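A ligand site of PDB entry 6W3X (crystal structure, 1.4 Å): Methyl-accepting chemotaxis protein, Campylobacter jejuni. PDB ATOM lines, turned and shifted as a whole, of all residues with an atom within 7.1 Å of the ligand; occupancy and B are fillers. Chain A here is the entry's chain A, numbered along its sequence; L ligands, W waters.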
ATOM      1  N   ASN A  80     -19.543  22.635 -27.708  1.00  0.00           N
ATOM      2  CA  ASN A  80     -19.337  22.032 -26.386  1.00  0.00           C
ATOM      3  C   ASN A  80     -20.664  21.502 -25.917  1.00  0.00           C
ATOM      4  O   ASN A  80     -21.704  22.188 -26.130  1.00  0.00           O
ATOM      5  CB  ASN A  80     -18.809  23.023 -25.314  1.00  0.00           C
ATOM      6  CG  ASN A  80     -17.487  23.638 -25.657  1.00  0.00           C
ATOM      7  OD1 ASN A  80     -16.457  22.954 -25.741  1.00  0.00           O
ATOM      8  ND2 ASN A  80     -17.511  24.966 -25.821  1.00  0.00           N
ATOM      9  N   VAL A  81     -20.658  20.362 -25.219  1.00  0.00           N
ATOM     10  CA  VAL A  81     -21.852  19.862 -24.528  1.00  0.00           C
ATOM     11  C   VAL A  81     -21.330  19.365 -23.171  1.00  0.00           C
ATOM     12  O   VAL A  81     -20.320  18.649 -23.112  1.00  0.00           O
ATOM     13  CB  VAL A  81     -22.533  18.751 -25.325  1.00  0.00           C
ATOM     14  CG1 VAL A  81     -23.702  18.170 -24.548  1.00  0.00           C
ATOM     15  CG2 VAL A  81     -22.997  19.233 -26.686  1.00  0.00           C
ATOM     16  N   TYR A  82     -22.006  19.765 -22.100  1.00  0.00           N
ATOM     17  CA  TYR A  82     -21.379  19.610 -20.786  1.00  0.00           C
ATOM     18  C   TYR A  82     -22.428  19.525 -19.684  1.00  0.00           C
ATOM     19  O   TYR A  82     -23.575  19.939 -19.840  1.00  0.00           O
ATOM     20  CB  TYR A  82     -20.380  20.766 -20.552  1.00  0.00           C
ATOM     21  CG  TYR A  82     -20.895  22.137 -20.862  1.00  0.00           C
ATOM     22  CD1 TYR A  82     -20.833  22.624 -22.153  1.00  0.00           C
ATOM     23  CD2 TYR A  82     -21.382  22.986 -19.867  1.00  0.00           C
ATOM     24  CE1 TYR A  82     -21.256  23.916 -22.451  1.00  0.00           C
ATOM     25  CE2 TYR A  82     -21.828  24.268 -20.133  1.00  0.00           C
ATOM     26  CZ  TYR A  82     -21.705  24.754 -21.445  1.00  0.00           C
ATOM     27  OH  TYR A  82     -22.077  26.044 -21.689  1.00  0.00           O
ATOM     28  N   VAL A  90     -17.152  20.365 -14.033  1.00  0.00           N
ATOM     29  CA  VAL A  90     -17.992  20.258 -15.227  1.00  0.00           C
ATOM     30  C   VAL A  90     -17.463  19.152 -16.123  1.00  0.00           C
ATOM     31  O   VAL A  90     -16.251  19.140 -16.484  1.00  0.00           O
ATOM     32  CB  VAL A  90     -18.126  21.615 -15.949  1.00  0.00           C
ATOM     33  CG1 VAL A  90     -16.772  22.167 -16.372  1.00  0.00           C
ATOM     34  CG2 VAL A  90     -19.027  21.514 -17.162  1.00  0.00           C
ATOM     35  N   LEU A  92     -17.079  17.810 -19.496  1.00  0.00           N
ATOM     36  CA  LEU A  92     -17.033  18.591 -20.750  1.00  0.00           C
ATOM     37  C   LEU A  92     -16.725  17.709 -21.939  1.00  0.00           C
ATOM     38  O   LEU A  92     -15.657  17.081 -21.989  1.00  0.00           O
ATOM     39  CB  LEU A  92     -15.997  19.709 -20.610  1.00  0.00           C
ATOM     40  CG  LEU A  92     -15.668  20.545 -21.830  1.00  0.00           C
ATOM     41  CD1 LEU A  92     -16.886  21.283 -22.336  1.00  0.00           C
ATOM     42  CD2 LEU A  92     -14.531  21.491 -21.508  1.00  0.00           C
ATOM     43  N   LEU A 108     -13.259  25.919 -14.384  1.00  0.00           N
ATOM     44  CA  LEU A 108     -14.102  26.744 -15.268  1.00  0.00           C
ATOM     45  C   LEU A 108     -15.063  27.679 -14.525  1.00  0.00           C
ATOM     46  O   LEU A 108     -15.872  28.370 -15.139  1.00  0.00           O
ATOM     47  CB  LEU A 108     -14.833  25.893 -16.311  1.00  0.00           C
ATOM     48  CG  LEU A 108     -13.875  25.215 -17.309  1.00  0.00           C
ATOM     49  CD1 LEU A 108     -14.553  24.147 -18.124  1.00  0.00           C
ATOM     50  CD2 LEU A 108     -13.040  26.165 -18.141  1.00  0.00           C
ATOM     51  N   ASP A 109     -14.919  27.777 -13.204  1.00  0.00           N
ATOM     52  CA  ASP A 109     -15.620  28.816 -12.419  1.00  0.00           C
ATOM     53  C   ASP A 109     -17.092  28.870 -12.746  1.00  0.00           C
ATOM     54  O   ASP A 109     -17.686  29.943 -12.917  1.00  0.00           O
ATOM     55  CB  ASP A 109     -14.999  30.202 -12.609  1.00  0.00           C
ATOM     56  CG  ASP A 109     -13.559  30.275 -12.171  1.00  0.00           C
ATOM     57  OD1 ASP A 109     -13.230  29.720 -11.109  1.00  0.00           O
ATOM     58  OD2 ASP A 109     -12.762  30.931 -12.880  1.00  0.00           O
ATOM     59  N   ILE A 110     -17.737  27.700 -12.692  1.00  0.00           N
ATOM     60  CA  ILE A 110     -19.030  27.579 -13.301  1.00  0.00           C
ATOM     61  C   ILE A 110     -20.104  28.289 -12.485  1.00  0.00           C
ATOM     62  O   ILE A 110     -21.056  28.776 -13.067  1.00  0.00           O
ATOM     63  CB  ILE A 110     -19.452  26.145 -13.598  1.00  0.00           C
ATOM     64  CG1 ILE A 110     -19.649  25.351 -12.301  1.00  0.00           C
ATOM     65  CG2 ILE A 110     -18.447  25.493 -14.521  1.00  0.00           C
ATOM     66  CD1 ILE A 110     -20.054  23.924 -12.577  1.00  0.00           C
ATOM     67  N   LYS A 113     -21.040  31.698 -13.680  1.00  0.00           N
ATOM     68  CA  LYS A 113     -21.548  31.828 -15.055  1.00  0.00           C
ATOM     69  C   LYS A 113     -23.068  31.952 -15.073  1.00  0.00           C
ATOM     70  O   LYS A 113     -23.783  31.195 -14.422  1.00  0.00           O
ATOM     71  CB  LYS A 113     -21.091  30.630 -15.894  1.00  0.00           C
ATOM     72  CG  LYS A 113     -19.601  30.320 -15.944  1.00  0.00           C
ATOM     73  CD  LYS A 113     -18.889  31.395 -16.702  1.00  0.00           C
ATOM     74  CE  LYS A 113     -17.381  31.268 -16.672  1.00  0.00           C
ATOM     75  NZ  LYS A 113     -16.858  30.042 -17.318  1.00  0.00           N
ATOM     76  N   ASP A 114     -23.589  32.797 -15.952  1.00  0.00           N
ATOM     77  CA  ASP A 114     -25.028  32.956 -16.079  1.00  0.00           C
ATOM     78  C   ASP A 114     -25.683  31.674 -16.584  1.00  0.00           C
ATOM     79  O   ASP A 114     -26.779  31.315 -16.141  1.00  0.00           O
ATOM     80  CB  ASP A 114     -25.378  34.106 -17.004  1.00  0.00           C
ATOM     81  CG  ASP A 114     -25.318  35.479 -16.291  1.00  0.00           C
ATOM     82  OD1 ASP A 114     -25.065  35.567 -15.056  1.00  0.00           O
ATOM     83  OD2 ASP A 114     -25.619  36.454 -16.961  1.00  0.00           O
ATOM     84  N   TRP A 115     -25.040  30.935 -17.463  1.00  0.00           N
ATOM     85  CA  TRP A 115     -25.690  29.703 -17.964  1.00  0.00           C
ATOM     86  C   TRP A 115     -25.972  28.759 -16.798  1.00  0.00           C
ATOM     87  O   TRP A 115     -26.958  27.984 -16.833  1.00  0.00           O
ATOM     88  CB  TRP A 115     -24.859  29.010 -19.052  1.00  0.00           C
ATOM     89  CG  TRP A 115     -23.496  28.476 -18.695  1.00  0.00           C
ATOM     90  CD1 TRP A 115     -22.308  29.045 -18.987  1.00  0.00           C
ATOM     91  CD2 TRP A 115     -23.191  27.277 -17.981  1.00  0.00           C
ATOM     92  NE1 TRP A 115     -21.257  28.304 -18.496  1.00  0.00           N
ATOM     93  CE2 TRP A 115     -21.792  27.213 -17.848  1.00  0.00           C
ATOM     94  CE3 TRP A 115     -23.961  26.205 -17.501  1.00  0.00           C
ATOM     95  CZ2 TRP A 115     -21.165  26.176 -17.222  1.00  0.00           C
ATOM     96  CZ3 TRP A 115     -23.328  25.138 -16.896  1.00  0.00           C
ATOM     97  CH2 TRP A 115     -21.934  25.171 -16.719  1.00  0.00           C
ATOM     98  N   TYR A 131     -21.738  35.081 -26.305  1.00  0.00           N
ATOM     99  CA  TYR A 131     -20.571  35.433 -25.470  1.00  0.00           C
ATOM    100  C   TYR A 131     -19.403  34.583 -25.910  1.00  0.00           C
ATOM    101  O   TYR A 131     -19.565  33.547 -26.579  1.00  0.00           O
ATOM    102  CB  TYR A 131     -20.861  35.281 -23.976  1.00  0.00           C
ATOM    103  CG  TYR A 131     -20.997  33.856 -23.540  1.00  0.00           C
ATOM    104  CD1 TYR A 131     -22.199  33.173 -23.689  1.00  0.00           C
ATOM    105  CD2 TYR A 131     -19.908  33.171 -23.015  1.00  0.00           C
ATOM    106  CE1 TYR A 131     -22.303  31.837 -23.388  1.00  0.00           C
ATOM    107  CE2 TYR A 131     -20.003  31.844 -22.650  1.00  0.00           C
ATOM    108  CZ  TYR A 131     -21.156  31.158 -22.903  1.00  0.00           C
ATOM    109  OH  TYR A 131     -21.236  29.824 -22.585  1.00  0.00           O
ATOM    110  N   LEU A 132     -18.198  34.988 -25.460  1.00  0.00           N
ATOM    111  CA  LEU A 132     -16.983  34.273 -25.789  1.00  0.00           C
ATOM    112  C   LEU A 132     -16.747  33.086 -24.910  1.00  0.00           C
ATOM    113  O   LEU A 132     -16.467  33.226 -23.716  1.00  0.00           O
ATOM    114  CB  LEU A 132     -15.803  35.214 -25.700  1.00  0.00           C
ATOM    115  CG  LEU A 132     -14.476  34.695 -26.261  1.00  0.00           C
ATOM    116  CD1 LEU A 132     -14.517  34.362 -27.730  1.00  0.00           C
ATOM    117  CD2 LEU A 132     -13.388  35.714 -26.002  1.00  0.00           C
ATOM    118  N   ASP A 133     -16.960  31.896 -25.450  1.00  0.00           N
ATOM    119  CA  ASP A 133     -16.717  30.678 -24.679  1.00  0.00           C
ATOM    120  C   ASP A 133     -15.292  30.630 -24.193  1.00  0.00           C
ATOM    121  O   ASP A 133     -14.350  30.802 -24.991  1.00  0.00           O
ATOM    122  CB  ASP A 133     -16.983  29.472 -25.600  1.00  0.00           C
ATOM    123  CG  ASP A 133     -16.420  28.180 -25.101  1.00  0.00           C
ATOM    124  OD1 ASP A 133     -16.583  27.890 -23.888  1.00  0.00           O
ATOM    125  OD2 ASP A 133     -15.821  27.449 -25.938  1.00  0.00           O
ATOM    126  N   THR A 134     -15.099  30.290 -22.919  1.00  0.00           N
ATOM    127  CA  THR A 134     -13.727  30.173 -22.382  1.00  0.00           C
ATOM    128  C   THR A 134     -12.944  28.982 -22.912  1.00  0.00           C
ATOM    129  O   THR A 134     -11.701  29.007 -22.978  1.00  0.00           O
ATOM    130  CB  THR A 134     -13.713  30.224 -20.851  1.00  0.00           C
ATOM    131  OG1 THR A 134     -14.454  29.131 -20.329  1.00  0.00           O
ATOM    132  CG2 THR A 134     -14.379  31.477 -20.374  1.00  0.00           C
ATOM    133  N   VAL A 135     -13.637  27.900 -23.280  1.00  0.00           N
ATOM    134  CA  VAL A 135     -12.960  26.674 -23.633  1.00  0.00           C
ATOM    135  C   VAL A 135     -12.289  26.739 -25.008  1.00  0.00           C
ATOM    136  O   VAL A 135     -11.091  26.597 -25.176  1.00  0.00           O
ATOM    137  CB  VAL A 135     -13.918  25.460 -23.487  1.00  0.00           C
ATOM    138  CG1 VAL A 135     -13.249  24.167 -24.000  1.00  0.00           C
ATOM    139  CG2 VAL A 135     -14.327  25.262 -22.031  1.00  0.00           C
ATOM    140  N   LEU A 136     -13.108  27.003 -25.997  1.00  0.00           N
ATOM    141  CA  LEU A 136     -12.679  27.040 -27.371  1.00  0.00           C
ATOM    142  C   LEU A 136     -12.602  28.436 -27.967  1.00  0.00           C
ATOM    143  O   LEU A 136     -12.186  28.590 -29.109  1.00  0.00           O
ATOM    144  CB  LEU A 136     -13.528  26.106 -28.229  1.00  0.00           C
ATOM    145  CG  LEU A 136     -13.245  24.632 -27.967  1.00  0.00           C
ATOM    146  CD1 LEU A 136     -14.245  23.740 -28.679  1.00  0.00           C
ATOM    147  CD2 LEU A 136     -11.843  24.256 -28.375  1.00  0.00           C
ATOM    148  N   GLN A 138     -14.562  30.782 -29.019  1.00  0.00           N
ATOM    149  CA  GLN A 138     -15.474  31.210 -30.097  1.00  0.00           C
ATOM    150  C   GLN A 138     -16.701  31.816 -29.461  1.00  0.00           C
ATOM    151  O   GLN A 138     -17.066  31.445 -28.336  1.00  0.00           O
ATOM    152  CB  GLN A 138     -15.868  30.044 -31.004  1.00  0.00           C
ATOM    153  CG  GLN A 138     -14.700  29.490 -31.773  1.00  0.00           C
ATOM    154  CD  GLN A 138     -15.075  28.329 -32.649  1.00  0.00           C
ATOM    155  OE1 GLN A 138     -16.171  28.322 -33.243  1.00  0.00           O
ATOM    156  NE2 GLN A 138     -14.212  27.324 -32.704  1.00  0.00           N
ATOM    157  N   VAL A 140     -20.511  31.986 -28.760  1.00  0.00           N
ATOM    158  CA  VAL A 140     -21.515  30.913 -28.678  1.00  0.00           C
ATOM    159  C   VAL A 140     -22.774  31.500 -28.074  1.00  0.00           C
ATOM    160  O   VAL A 140     -22.759  32.490 -27.353  1.00  0.00           O
ATOM    161  CB  VAL A 140     -21.031  29.739 -27.816  1.00  0.00           C
ATOM    162  CG1 VAL A 140     -19.792  29.117 -28.428  1.00  0.00           C
ATOM    163  CG2 VAL A 140     -20.881  30.076 -26.342  1.00  0.00           C
ATOM    164  N   THR A 142     -25.476  29.754 -25.585  1.00  0.00           N
ATOM    165  CA  THR A 142     -25.600  28.587 -24.713  1.00  0.00           C
ATOM    166  C   THR A 142     -27.049  28.350 -24.340  1.00  0.00           C
ATOM    167  O   THR A 142     -27.769  29.271 -23.942  1.00  0.00           O
ATOM    168  CB  THR A 142     -24.701  28.725 -23.455  1.00  0.00           C
ATOM    169  OG1 THR A 142     -23.329  28.837 -23.899  1.00  0.00           O
ATOM    170  CG2 THR A 142     -24.901  27.586 -22.464  1.00  0.00           C
ATOM    171  N   ASP A 160     -23.346  24.520 -26.248  1.00  0.00           N
ATOM    172  CA  ASP A 160     -22.822  25.735 -26.885  1.00  0.00           C
ATOM    173  C   ASP A 160     -22.895  25.584 -28.406  1.00  0.00           C
ATOM    174  O   ASP A 160     -22.291  24.647 -28.960  1.00  0.00           O
ATOM    175  CB  ASP A 160     -21.343  25.965 -26.518  1.00  0.00           C
ATOM    176  CG  ASP A 160     -21.105  26.317 -25.065  1.00  0.00           C
ATOM    177  OD1 ASP A 160     -22.084  26.589 -24.325  1.00  0.00           O
ATOM    178  OD2 ASP A 160     -19.916  26.298 -24.709  1.00  0.00           O
HETATM  179  N1  LIG L   1     -19.027  27.961 -22.633  1.00  0.00           N
HETATM  180  C1  LIG L   1     -18.860  27.661 -21.192  1.00  0.00           C
HETATM  181  C2  LIG L   1     -18.377  28.931 -20.512  1.00  0.00           C
HETATM  182  O1  LIG L   1     -17.672  29.687 -21.182  1.00  0.00           O
HETATM  183  C3  LIG L   1     -17.846  26.525 -20.922  1.00  0.00           C
HETATM  184  C4  LIG L   1     -17.943  26.048 -19.483  1.00  0.00           C
HETATM  185  C5  LIG L   1     -18.076  25.304 -21.800  1.00  0.00           C
HETATM  186  O2  LIG L   1     -18.661  29.136 -19.327  1.00  0.00           O
HETATM  187  O   HOH W   1     -17.210  32.267 -20.138  1.00  0.00           O
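The side-chain carboxylate of Asp 160 is in hydrogen-bond range of the side-chain hydroxyl of Tyr 82, at 2.7 Å. O of Tyr 131 is in hydrogen-bond range of N of Val 140. OH of Tyr 131 lies within hydrogen-bond range of OG1 of Thr 142, 2.7 Å away. The side-chain carboxylate (OD1) of Asp 133 lies within hydrogen-bond range of the backbone NH (N) of Val 135 (3.0 Å). N of Asp 160 is in hydrogen-bond range of O of Asn 80, at 2.9 Å. ND2 of Asn 80 is in hydrogen-bond range of OD2 of Asp 133, 3.0 Å away. O of Leu 108 lies within hydrogen-bond range of NZ of Lys 113, 2.9 Å away. The side-chain carboxylate (OD1) of Asp 160 is in hydrogen-bond range of the side-chain hydroxyl (OG1) of Thr 142.
An oxygen (O1) of the ligand lies within hydrogen-bond range of the backbone NH (N) of Thr 134, 3.2 Å away. The side-chain hydroxyl of Thr 134 is in hydrogen-bond range of an oxygen (O1) of the ligand (3.4 Å). A nitrogen (N1) of the ligand is in salt-bridge range of the side-chain carboxylate (OD2) of Asp 160, at 2.8 Å. N1 of the ligand is in hydrogen-bond range of OH of Tyr 131 (2.9 Å). NE1 of Trp 115 is in hydrogen-bond range of O2 of the ligand. The side-chain amino group of Lys 113 lies within salt-bridge range of an oxygen (O2) of the ligand, at 2.8 Å. A nitrogen (N1) of the ligand is in salt-bridge range of the side-chain carboxylate of Asp 133, at 2.7 Å.
Merely in contact with the ligand: Tyr 82 and Val 135. Of the 21 residues printed, 8 come within 4 Å of the ligand.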
